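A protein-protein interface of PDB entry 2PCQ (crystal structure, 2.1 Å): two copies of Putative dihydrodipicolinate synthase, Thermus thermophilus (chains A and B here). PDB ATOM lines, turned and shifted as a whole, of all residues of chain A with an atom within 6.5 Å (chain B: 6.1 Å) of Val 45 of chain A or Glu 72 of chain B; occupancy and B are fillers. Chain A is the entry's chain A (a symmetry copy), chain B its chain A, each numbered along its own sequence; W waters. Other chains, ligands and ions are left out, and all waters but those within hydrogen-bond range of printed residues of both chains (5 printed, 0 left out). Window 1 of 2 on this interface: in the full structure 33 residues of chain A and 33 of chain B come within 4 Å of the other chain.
Among the printed residues, merely in contact across the chains: Val 45 of chain A with Glu 72 of chain B (3.7 Å), Val 45 of chain A with Tyr 99 of chain B (3.7 Å), His 46 of chain A with Glu 72 of chain B (3.4 Å), His 46 of chain A with Thr 73 of chain B (3.3 Å), His 46 of chain A with Tyr 100 of chain B (3.3 Å), Arg 256 of chain A with Thr 73 of chain B (3.8 Å), Pro 257 of chain A with Thr 73 of chain B (3.1 Å), Pro 258 of chain A with Thr 73 of chain B (3.9 Å), Pro 258 of chain A with Leu 74 of chain B (3.8 Å), Pro 258 of chain A with Tyr 111 of chain B (3.8 Å), Tyr 259 of chain A with Glu 72 of chain B (3.8 Å), Tyr 259 of chain A with Pro 97 of chain B (3.5 Å) and Tyr 259 of chain A with Tyr 100 of chain B (3.1 Å).
Printed residues of chain B that touch a printed residue of chain A: Glu 72, Thr 73, Leu 74, Gln 76, Pro 97, Tyr 99, Tyr 100 and Tyr 111. Hydrophobic or aromatic side chains of chain B within 4 Å of the printed part of chain A: Pro 97, Tyr 99, Tyr 100 and Tyr 111. Hydrophobic or aromatic side chains of chain A that line the printed part of chain B: Val 45, His 46, Met 70, Pro 258 and Tyr 259.
The backbone carbonyl oxygen of Pro 257 of chain A lies within hydrogen-bond range of the backbone NH of Leu 74 of chain B (3.1 Å). The side-chain amide nitrogen (NE2) of Gln 76 of chain B is in hydrogen-bond range of the backbone carbonyl oxygen (O) of Val 45 of chain A (3.1 Å). OH of Tyr 99 of chain B lies within hydrogen-bond range of SD of Met 70 of chain A (3.1 Å). N of Glu 43 of chain A is in hydrogen-bond range of OH of Tyr 100 of chain B (3.0 Å). The side-chain amide oxygen (OE1) of Gln 76 of chain B lies close to the backbone carbonyl oxygen (O) of His 46 of chain A (3.4 Å). The side-chain amide nitrogen (NE2) of Gln 76 of chain B lies close to the backbone NH (N) of Leu 47 of chain A.
Water W1 lies within hydrogen-bond range of OH of Tyr 259 of chain A, NE2 of His 46 of chain A, OE1 of Glu 72 of chain B and N of Tyr 100 of chain B. Water W3 lies within hydrogen-bond range of the guanidinium group of Arg 98 of chain A (2.7 Å) and the side-chain carboxylate of Glu 72 of chain B (2.9 Å). Water W2 bridges the guanidinium group (NH1) of Arg 98 of chain B (2.7 Å) and the side-chain carboxylate (OE2) of Glu 72 of chain A (2.9 Å). Water W4 lies within hydrogen-bond range of OH of Tyr 100 of chain B (2.9 Å), N of Gly 44 of chain A (3.0 Å) and N of Val 45 of chain A (3.0 Å). Water W5 bridges the side-chain amide nitrogen (NE2) of Gln 76 of chain B and the backbone carbonyl oxygen (O) of Leu 47 of chain A.
The side-chain carboxylate (OE1) of Glu 43 of chain A sits at hydrogen-bond distance from a ring nitrogen (ND1) of His 46 of chain A. N of Arg 256 of chain A sits at hydrogen-bond distance from OE1 of Glu 43 of chain A, at 3.1 Å. The guanidinium group (NH1) of Arg 256 of chain A is in hydrogen-bond range of the backbone carbonyl oxygen (O) of His 46 of chain A (2.7 Å). The guanidinium group of Arg 98 of chain B is in salt-bridge range of the side-chain carboxylate of Glu 72 of chain B (3.6 Å). The guanidinium group of Arg 98 of chain A lies within hydrogen-bond range of the backbone carbonyl oxygen of Met 70 of chain A. OE1 of Glu 72 of chain B sits at hydrogen-bond distance from N of Tyr 99 of chain B (3.0 Å).
Positions printed for both chains: 70, 71, 72 and 98.
Of the printed residues of chain B, Val 45 of chain A touches Glu 72, Gln 76 and Tyr 99. Printed residues of chain B within 4 Å of Arg 256 of chain A: Thr 73. Of chain A, only Val 45, His 46 and Tyr 259 come within 4 Å of Glu 72 of chain B. Of the printed residues of chain A, Gln 76 of chain B touches Val 45 (3.1 Å), His 46 (3.2 Å) and Leu 47 (3.5 Å). Ala 77 of chain B touches none of the printed residues of chain A. Of the printed residues of chain A, Tyr 111 of chain B touches Pro 258.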
ATOM      1  N   GLY A  39      17.144 -14.090  23.596  1.00  0.00           N
ATOM      2  CA  GLY A  39      15.823 -13.488  23.646  1.00  0.00           C
ATOM      3  C   GLY A  39      16.052 -11.990  23.540  1.00  0.00           C
ATOM      4  O   GLY A  39      17.184 -11.572  23.305  1.00  0.00           O
ATOM      5  N   GLY A  42      18.742 -10.871  25.603  1.00  0.00           N
ATOM      6  CA  GLY A  42      19.993 -11.574  25.359  1.00  0.00           C
ATOM      7  C   GLY A  42      21.011 -10.944  24.421  1.00  0.00           C
ATOM      8  O   GLY A  42      22.038 -11.557  24.136  1.00  0.00           O
ATOM      9  N   GLU A  43      20.736  -9.733  23.940  1.00  0.00           N
ATOM     10  CA  GLU A  43      21.637  -9.015  23.038  1.00  0.00           C
ATOM     11  C   GLU A  43      22.058  -9.796  21.798  1.00  0.00           C
ATOM     12  O   GLU A  43      23.187  -9.667  21.322  1.00  0.00           O
ATOM     13  CB  GLU A  43      22.885  -8.540  23.797  1.00  0.00           C
ATOM     14  CG  GLU A  43      22.588  -7.439  24.810  1.00  0.00           C
ATOM     15  CD  GLU A  43      23.823  -6.961  25.556  1.00  0.00           C
ATOM     16  OE1 GLU A  43      24.613  -6.181  24.982  1.00  0.00           O
ATOM     17  OE2 GLU A  43      24.003  -7.371  26.722  1.00  0.00           O
ATOM     18  N   GLY A  44      21.142 -10.597  21.267  1.00  0.00           N
ATOM     19  CA  GLY A  44      21.452 -11.357  20.074  1.00  0.00           C
ATOM     20  C   GLY A  44      21.846 -10.452  18.917  1.00  0.00           C
ATOM     21  O   GLY A  44      22.765 -10.773  18.169  1.00  0.00           O
ATOM     22  N   VAL A  45      21.163  -9.318  18.770  1.00  0.00           N
ATOM     23  CA  VAL A  45      21.466  -8.387  17.682  1.00  0.00           C
ATOM     24  C   VAL A  45      22.785  -7.649  17.882  1.00  0.00           C
ATOM     25  O   VAL A  45      23.225  -6.907  17.004  1.00  0.00           O
ATOM     26  CB  VAL A  45      20.339  -7.342  17.480  1.00  0.00           C
ATOM     27  CG1 VAL A  45      19.034  -8.050  17.126  1.00  0.00           C
ATOM     28  CG2 VAL A  45      20.174  -6.495  18.731  1.00  0.00           C
ATOM     29  N   HIS A  46      23.418  -7.851  19.035  1.00  0.00           N
ATOM     30  CA  HIS A  46      24.700  -7.215  19.307  1.00  0.00           C
ATOM     31  C   HIS A  46      25.854  -8.133  18.907  1.00  0.00           C
ATOM     32  O   HIS A  46      27.021  -7.796  19.094  1.00  0.00           O
ATOM     33  CB  HIS A  46      24.816  -6.851  20.789  1.00  0.00           C
ATOM     34  CG  HIS A  46      24.054  -5.620  21.168  1.00  0.00           C
ATOM     35  ND1 HIS A  46      24.086  -5.089  22.441  1.00  0.00           N
ATOM     36  CD2 HIS A  46      23.270  -4.793  20.436  1.00  0.00           C
ATOM     37  CE1 HIS A  46      23.358  -3.988  22.474  1.00  0.00           C
ATOM     38  NE2 HIS A  46      22.851  -3.785  21.271  1.00  0.00           N
ATOM     39  N   LEU A  47      25.517  -9.287  18.340  1.00  0.00           N
ATOM     40  CA  LEU A  47      26.524 -10.259  17.922  1.00  0.00           C
ATOM     41  C   LEU A  47      26.591 -10.414  16.411  1.00  0.00           C
ATOM     42  O   LEU A  47      25.585 -10.273  15.722  1.00  0.00           O
ATOM     43  CB  LEU A  47      26.209 -11.634  18.517  1.00  0.00           C
ATOM     44  CG  LEU A  47      26.054 -11.771  20.031  1.00  0.00           C
ATOM     45  CD1 LEU A  47      25.523 -13.155  20.355  1.00  0.00           C
ATOM     46  CD2 LEU A  47      27.388 -11.531  20.710  1.00  0.00           C
ATOM     47  N   THR A  48      27.782 -10.710  15.903  1.00  0.00           N
ATOM     48  CA  THR A  48      27.955 -10.951  14.477  1.00  0.00           C
ATOM     49  C   THR A  48      27.531 -12.408  14.293  1.00  0.00           C
ATOM     50  O   THR A  48      27.451 -13.155  15.267  1.00  0.00           O
ATOM     51  CB  THR A  48      29.431 -10.826  14.043  1.00  0.00           C
ATOM     52  OG1 THR A  48      30.216 -11.801  14.738  1.00  0.00           O
ATOM     53  CG2 THR A  48      29.962  -9.435  14.341  1.00  0.00           C
ATOM     54  N   MET A  70      16.450 -13.165  15.433  1.00  0.00           N
ATOM     55  CA  MET A  70      16.109 -11.820  15.015  1.00  0.00           C
ATOM     56  C   MET A  70      16.976 -11.384  13.840  1.00  0.00           C
ATOM     57  O   MET A  70      18.103 -10.916  14.020  1.00  0.00           O
ATOM     58  CB  MET A  70      16.288 -10.865  16.181  1.00  0.00           C
ATOM     59  CG  MET A  70      15.591 -11.359  17.420  1.00  0.00           C
ATOM     60  SD  MET A  70      15.691 -10.099  18.843  1.00  0.00           S
ATOM     61  CE  MET A  70      15.100 -11.270  20.270  1.00  0.00           C
ATOM     62  N   GLU A  71      16.440 -11.562  12.635  1.00  0.00           N
ATOM     63  CA  GLU A  71      17.138 -11.202  11.408  1.00  0.00           C
ATOM     64  C   GLU A  71      16.208 -10.350  10.552  1.00  0.00           C
ATOM     65  O   GLU A  71      14.999 -10.293  10.795  1.00  0.00           O
ATOM     66  CB  GLU A  71      17.556 -12.453  10.628  1.00  0.00           C
ATOM     67  CG  GLU A  71      18.508 -13.398  11.357  1.00  0.00           C
ATOM     68  CD  GLU A  71      19.814 -12.740  11.772  1.00  0.00           C
ATOM     69  OE1 GLU A  71      20.322 -11.874  11.029  1.00  0.00           O
ATOM     70  OE2 GLU A  71      20.343 -13.103  12.845  1.00  0.00           O
ATOM     71  N   GLU A  72      16.780  -9.699   9.545  1.00  0.00           N
ATOM     72  CA  GLU A  72      16.029  -8.827   8.654  1.00  0.00           C
ATOM     73  C   GLU A  72      15.599  -9.532   7.373  1.00  0.00           C
ATOM     74  O   GLU A  72      14.650  -9.102   6.726  1.00  0.00           O
ATOM     75  CB  GLU A  72      16.874  -7.608   8.278  1.00  0.00           C
ATOM     76  CG  GLU A  72      17.431  -6.800   9.452  1.00  0.00           C
ATOM     77  CD  GLU A  72      16.430  -5.813  10.043  1.00  0.00           C
ATOM     78  OE1 GLU A  72      15.291  -5.720   9.531  1.00  0.00           O
ATOM     79  OE2 GLU A  72      16.791  -5.126  11.025  1.00  0.00           O
ATOM     80  N   ARG A  98      12.637  -5.808  10.583  1.00  0.00           N
ATOM     81  CA  ARG A  98      12.405  -4.465  11.130  1.00  0.00           C
ATOM     82  C   ARG A  98      12.658  -3.213  10.292  1.00  0.00           C
ATOM     83  O   ARG A  98      11.753  -2.405  10.070  1.00  0.00           O
ATOM     84  CB  ARG A  98      13.222  -4.295  12.410  1.00  0.00           C
ATOM     85  CG  ARG A  98      12.786  -5.135  13.584  1.00  0.00           C
ATOM     86  CD  ARG A  98      13.998  -5.418  14.445  1.00  0.00           C
ATOM     87  NE  ARG A  98      14.723  -6.563  13.920  1.00  0.00           N
ATOM     88  CZ  ARG A  98      16.038  -6.727  13.986  1.00  0.00           C
ATOM     89  NH1 ARG A  98      16.808  -5.808  14.554  1.00  0.00           N
ATOM     90  NH2 ARG A  98      16.574  -7.831  13.493  1.00  0.00           N
ATOM     91  N   ARG A 256      27.182  -4.696  25.849  1.00  0.00           N
ATOM     92  CA  ARG A 256      28.230  -4.384  24.887  1.00  0.00           C
ATOM     93  C   ARG A 256      28.285  -2.879  24.631  1.00  0.00           C
ATOM     94  O   ARG A 256      27.251  -2.245  24.431  1.00  0.00           O
ATOM     95  CB  ARG A 256      27.988  -5.142  23.577  1.00  0.00           C
ATOM     96  CG  ARG A 256      29.269  -5.442  22.823  1.00  0.00           C
ATOM     97  CD  ARG A 256      29.073  -6.422  21.666  1.00  0.00           C
ATOM     98  NE  ARG A 256      30.323  -7.134  21.416  1.00  0.00           N
ATOM     99  CZ  ARG A 256      30.556  -7.953  20.395  1.00  0.00           C
ATOM    100  NH1 ARG A 256      29.625  -8.190  19.481  1.00  0.00           N
ATOM    101  NH2 ARG A 256      31.737  -8.551  20.300  1.00  0.00           N
ATOM    102  N   PRO A 257      29.495  -2.282  24.660  1.00  0.00           N
ATOM    103  CA  PRO A 257      29.626  -0.839  24.422  1.00  0.00           C
ATOM    104  C   PRO A 257      28.907  -0.489  23.124  1.00  0.00           C
ATOM    105  O   PRO A 257      28.874  -1.299  22.196  1.00  0.00           O
ATOM    106  CB  PRO A 257      31.136  -0.641  24.322  1.00  0.00           C
ATOM    107  CG  PRO A 257      31.664  -1.692  25.266  1.00  0.00           C
ATOM    108  CD  PRO A 257      30.813  -2.895  24.910  1.00  0.00           C
ATOM    109  N   PRO A 258      28.379   0.740  23.013  1.00  0.00           N
ATOM    110  CA  PRO A 258      28.393   1.870  23.949  1.00  0.00           C
ATOM    111  C   PRO A 258      27.418   1.844  25.126  1.00  0.00           C
ATOM    112  O   PRO A 258      27.279   2.843  25.827  1.00  0.00           O
ATOM    113  CB  PRO A 258      28.118   3.047  23.034  1.00  0.00           C
ATOM    114  CG  PRO A 258      27.046   2.469  22.145  1.00  0.00           C
ATOM    115  CD  PRO A 258      27.583   1.081  21.816  1.00  0.00           C
ATOM    116  N   TYR A 259      26.734   0.732  25.348  1.00  0.00           N
ATOM    117  CA  TYR A 259      25.796   0.690  26.459  1.00  0.00           C
ATOM    118  C   TYR A 259      26.521   0.706  27.810  1.00  0.00           C
ATOM    119  O   TYR A 259      27.616   0.157  27.945  1.00  0.00           O
ATOM    120  CB  TYR A 259      24.864  -0.515  26.308  1.00  0.00           C
ATOM    121  CG  TYR A 259      23.903  -0.330  25.146  1.00  0.00           C
ATOM    122  CD1 TYR A 259      24.215  -0.795  23.864  1.00  0.00           C
ATOM    123  CD2 TYR A 259      22.708   0.370  25.317  1.00  0.00           C
ATOM    124  CE1 TYR A 259      23.356  -0.564  22.783  1.00  0.00           C
ATOM    125  CE2 TYR A 259      21.848   0.608  24.247  1.00  0.00           C
ATOM    126  CZ  TYR A 259      22.175   0.137  22.986  1.00  0.00           C
ATOM    127  OH  TYR A 259      21.310   0.363  21.940  1.00  0.00           O
ATOM    128  N   MET B  70      25.592   1.290   9.824  1.00  0.00           N
ATOM    129  CA  MET B  70      24.471   1.051  10.710  1.00  0.00           C
ATOM    130  C   MET B  70      24.695  -0.210  11.536  1.00  0.00           C
ATOM    131  O   MET B  70      24.421  -1.324  11.083  1.00  0.00           O
ATOM    132  CB  MET B  70      23.197   0.925   9.895  1.00  0.00           C
ATOM    133  CG  MET B  70      23.035   2.070   8.931  1.00  0.00           C
ATOM    134  SD  MET B  70      21.371   1.992   8.008  1.00  0.00           S
ATOM    135  CE  MET B  70      21.770   3.309   6.643  1.00  0.00           C
ATOM    136  N   GLU B  71      25.212  -0.019  12.747  1.00  0.00           N
ATOM    137  CA  GLU B  71      25.491  -1.117  13.661  1.00  0.00           C
ATOM    138  C   GLU B  71      24.868  -0.794  15.015  1.00  0.00           C
ATOM    139  O   GLU B  71      24.490   0.350  15.280  1.00  0.00           O
ATOM    140  CB  GLU B  71      27.001  -1.325  13.824  1.00  0.00           C
ATOM    141  CG  GLU B  71      27.760  -1.676  12.546  1.00  0.00           C
ATOM    142  CD  GLU B  71      27.261  -2.943  11.873  1.00  0.00           C
ATOM    143  OE1 GLU B  71      26.860  -3.892  12.582  1.00  0.00           O
ATOM    144  OE2 GLU B  71      27.281  -2.997  10.624  1.00  0.00           O
ATOM    145  N   GLU B  72      24.776  -1.809  15.868  1.00  0.00           N
ATOM    146  CA  GLU B  72      24.183  -1.663  17.189  1.00  0.00           C
ATOM    147  C   GLU B  72      25.227  -1.423  18.273  1.00  0.00           C
ATOM    148  O   GLU B  72      24.901  -0.888  19.328  1.00  0.00           O
ATOM    149  CB  GLU B  72      23.389  -2.921  17.548  1.00  0.00           C
ATOM    150  CG  GLU B  72      22.319  -3.341  16.539  1.00  0.00           C
ATOM    151  CD  GLU B  72      21.007  -2.577  16.688  1.00  0.00           C
ATOM    152  OE1 GLU B  72      20.898  -1.725  17.600  1.00  0.00           O
ATOM    153  OE2 GLU B  72      20.081  -2.836  15.887  1.00  0.00           O
ATOM    154  N   THR B  73      26.473  -1.819  18.021  1.00  0.00           N
ATOM    155  CA  THR B  73      27.533  -1.662  19.017  1.00  0.00           C
ATOM    156  C   THR B  73      28.878  -1.262  18.418  1.00  0.00           C
ATOM    157  O   THR B  73      29.098  -1.386  17.216  1.00  0.00           O
ATOM    158  CB  THR B  73      27.757  -2.970  19.795  1.00  0.00           C
ATOM    159  OG1 THR B  73      28.307  -3.962  18.914  1.00  0.00           O
ATOM    160  CG2 THR B  73      26.444  -3.485  20.363  1.00  0.00           C
ATOM    161  N   LEU B  74      29.779  -0.790  19.272  1.00  0.00           N
ATOM    162  CA  LEU B  74      31.102  -0.387  18.823  1.00  0.00           C
ATOM    163  C   LEU B  74      31.887  -1.579  18.272  1.00  0.00           C
ATOM    164  O   LEU B  74      32.527  -1.472  17.233  1.00  0.00           O
ATOM    165  CB  LEU B  74      31.861   0.295  19.966  1.00  0.00           C
ATOM    166  CG  LEU B  74      31.336   1.706  20.269  1.00  0.00           C
ATOM    167  CD1 LEU B  74      31.986   2.263  21.523  1.00  0.00           C
ATOM    168  CD2 LEU B  74      31.617   2.609  19.066  1.00  0.00           C
ATOM    169  N   GLN B  76      30.850  -4.183  16.740  1.00  0.00           N
ATOM    170  CA  GLN B  76      30.329  -4.487  15.407  1.00  0.00           C
ATOM    171  C   GLN B  76      30.670  -3.369  14.429  1.00  0.00           C
ATOM    172  O   GLN B  76      30.894  -3.613  13.247  1.00  0.00           O
ATOM    173  CB  GLN B  76      28.808  -4.663  15.448  1.00  0.00           C
ATOM    174  CG  GLN B  76      28.343  -5.944  16.112  1.00  0.00           C
ATOM    175  CD  GLN B  76      26.880  -5.892  16.488  1.00  0.00           C
ATOM    176  OE1 GLN B  76      26.457  -5.017  17.246  1.00  0.00           O
ATOM    177  NE2 GLN B  76      26.096  -6.827  15.963  1.00  0.00           N
ATOM    178  N   ALA B  77      30.702  -2.142  14.934  1.00  0.00           N
ATOM    179  CA  ALA B  77      31.010  -0.980  14.115  1.00  0.00           C
ATOM    180  C   ALA B  77      32.469  -0.938  13.661  1.00  0.00           C
ATOM    181  O   ALA B  77      32.767  -0.488  12.553  1.00  0.00           O
ATOM    182  CB  ALA B  77      30.677   0.291  14.883  1.00  0.00           C
ATOM    183  N   PRO B  96      22.293   5.945  14.903  1.00  0.00           N
ATOM    184  CA  PRO B  96      22.451   5.596  16.320  1.00  0.00           C
ATOM    185  C   PRO B  96      22.082   4.131  16.555  1.00  0.00           C
ATOM    186  O   PRO B  96      21.371   3.530  15.749  1.00  0.00           O
ATOM    187  CB  PRO B  96      21.447   6.517  17.023  1.00  0.00           C
ATOM    188  CG  PRO B  96      21.198   7.625  16.033  1.00  0.00           C
ATOM    189  CD  PRO B  96      21.188   6.898  14.720  1.00  0.00           C
ATOM    190  N   PRO B  97      22.586   3.528  17.645  1.00  0.00           N
ATOM    191  CA  PRO B  97      22.235   2.127  17.910  1.00  0.00           C
ATOM    192  C   PRO B  97      20.702   2.118  18.008  1.00  0.00           C
ATOM    193  O   PRO B  97      20.115   3.119  18.410  1.00  0.00           O
ATOM    194  CB  PRO B  97      22.913   1.855  19.250  1.00  0.00           C
ATOM    195  CG  PRO B  97      24.159   2.691  19.152  1.00  0.00           C
ATOM    196  CD  PRO B  97      23.634   3.996  18.572  1.00  0.00           C
ATOM    197  N   ARG B  98      20.061   1.004  17.667  1.00  0.00           N
ATOM    198  CA  ARG B  98      18.593   0.947  17.664  1.00  0.00           C
ATOM    199  C   ARG B  98      17.832   0.081  18.664  1.00  0.00           C
ATOM    200  O   ARG B  98      17.011   0.578  19.439  1.00  0.00           O
ATOM    201  CB  ARG B  98      18.109   0.526  16.277  1.00  0.00           C
ATOM    202  CG  ARG B  98      18.334   1.525  15.170  1.00  0.00           C
ATOM    203  CD  ARG B  98      18.496   0.769  13.870  1.00  0.00           C
ATOM    204  NE  ARG B  98      19.871   0.324  13.722  1.00  0.00           N
ATOM    205  CZ  ARG B  98      20.249  -0.793  13.114  1.00  0.00           C
ATOM    206  NH1 ARG B  98      19.351  -1.615  12.587  1.00  0.00           N
ATOM    207  NH2 ARG B  98      21.539  -1.071  13.022  1.00  0.00           N
ATOM    208  N   TYR B  99      18.079  -1.222  18.605  1.00  0.00           N
ATOM    209  CA  TYR B  99      17.370  -2.184  19.433  1.00  0.00           C
ATOM    210  C   TYR B  99      17.178  -1.820  20.909  1.00  0.00           C
ATOM    211  O   TYR B  99      16.059  -1.893  21.414  1.00  0.00           O
ATOM    212  CB  TYR B  99      18.037  -3.554  19.312  1.00  0.00           C
ATOM    213  CG  TYR B  99      17.116  -4.695  19.657  1.00  0.00           C
ATOM    214  CD1 TYR B  99      16.269  -5.252  18.697  1.00  0.00           C
ATOM    215  CD2 TYR B  99      17.073  -5.208  20.951  1.00  0.00           C
ATOM    216  CE1 TYR B  99      15.399  -6.297  19.023  1.00  0.00           C
ATOM    217  CE2 TYR B  99      16.207  -6.252  21.288  1.00  0.00           C
ATOM    218  CZ  TYR B  99      15.376  -6.789  20.323  1.00  0.00           C
ATOM    219  OH  TYR B  99      14.523  -7.813  20.662  1.00  0.00           O
ATOM    220  N   TYR B 100      18.250  -1.437  21.600  1.00  0.00           N
ATOM    221  CA  TYR B 100      18.146  -1.076  23.021  1.00  0.00           C
ATOM    222  C   TYR B 100      18.322   0.425  23.234  1.00  0.00           C
ATOM    223  O   TYR B 100      18.718   0.867  24.312  1.00  0.00           O
ATOM    224  CB  TYR B 100      19.211  -1.820  23.834  1.00  0.00           C
ATOM    225  CG  TYR B 100      19.128  -3.325  23.734  1.00  0.00           C
ATOM    226  CD1 TYR B 100      18.180  -4.044  24.463  1.00  0.00           C
ATOM    227  CD2 TYR B 100      19.982  -4.028  22.889  1.00  0.00           C
ATOM    228  CE1 TYR B 100      18.090  -5.431  24.346  1.00  0.00           C
ATOM    229  CE2 TYR B 100      19.899  -5.405  22.761  1.00  0.00           C
ATOM    230  CZ  TYR B 100      18.955  -6.101  23.490  1.00  0.00           C
ATOM    231  OH  TYR B 100      18.883  -7.464  23.351  1.00  0.00           O
ATOM    232  N   TYR B 111      29.229   6.684  21.483  1.00  0.00           N
ATOM    233  CA  TYR B 111      29.239   5.945  20.224  1.00  0.00           C
ATOM    234  C   TYR B 111      29.849   6.787  19.102  1.00  0.00           C
ATOM    235  O   TYR B 111      30.814   6.380  18.458  1.00  0.00           O
ATOM    236  CB  TYR B 111      27.810   5.539  19.846  1.00  0.00           C
ATOM    237  CG  TYR B 111      27.711   4.660  18.617  1.00  0.00           C
ATOM    238  CD1 TYR B 111      28.205   3.352  18.624  1.00  0.00           C
ATOM    239  CD2 TYR B 111      27.132   5.138  17.442  1.00  0.00           C
ATOM    240  CE1 TYR B 111      28.121   2.544  17.489  1.00  0.00           C
ATOM    241  CE2 TYR B 111      27.045   4.338  16.303  1.00  0.00           C
ATOM    242  CZ  TYR B 111      27.541   3.046  16.333  1.00  0.00           C
ATOM    243  OH  TYR B 111      27.456   2.264  15.209  1.00  0.00           O
HETATM  244  O   HOH W   1      21.223  -1.718  20.375  1.00  0.00           O
HETATM  245  O   HOH W   2      16.816  -2.623  12.423  1.00  0.00           O
HETATM  246  O   HOH W   3      17.289  -3.246  15.375  1.00  0.00           O
HETATM  247  O   HOH W   4      18.914  -8.719  20.707  1.00  0.00           O
HETATM  248  O   HOH W   5      26.262  -8.288  12.943  1.00  0.00           O
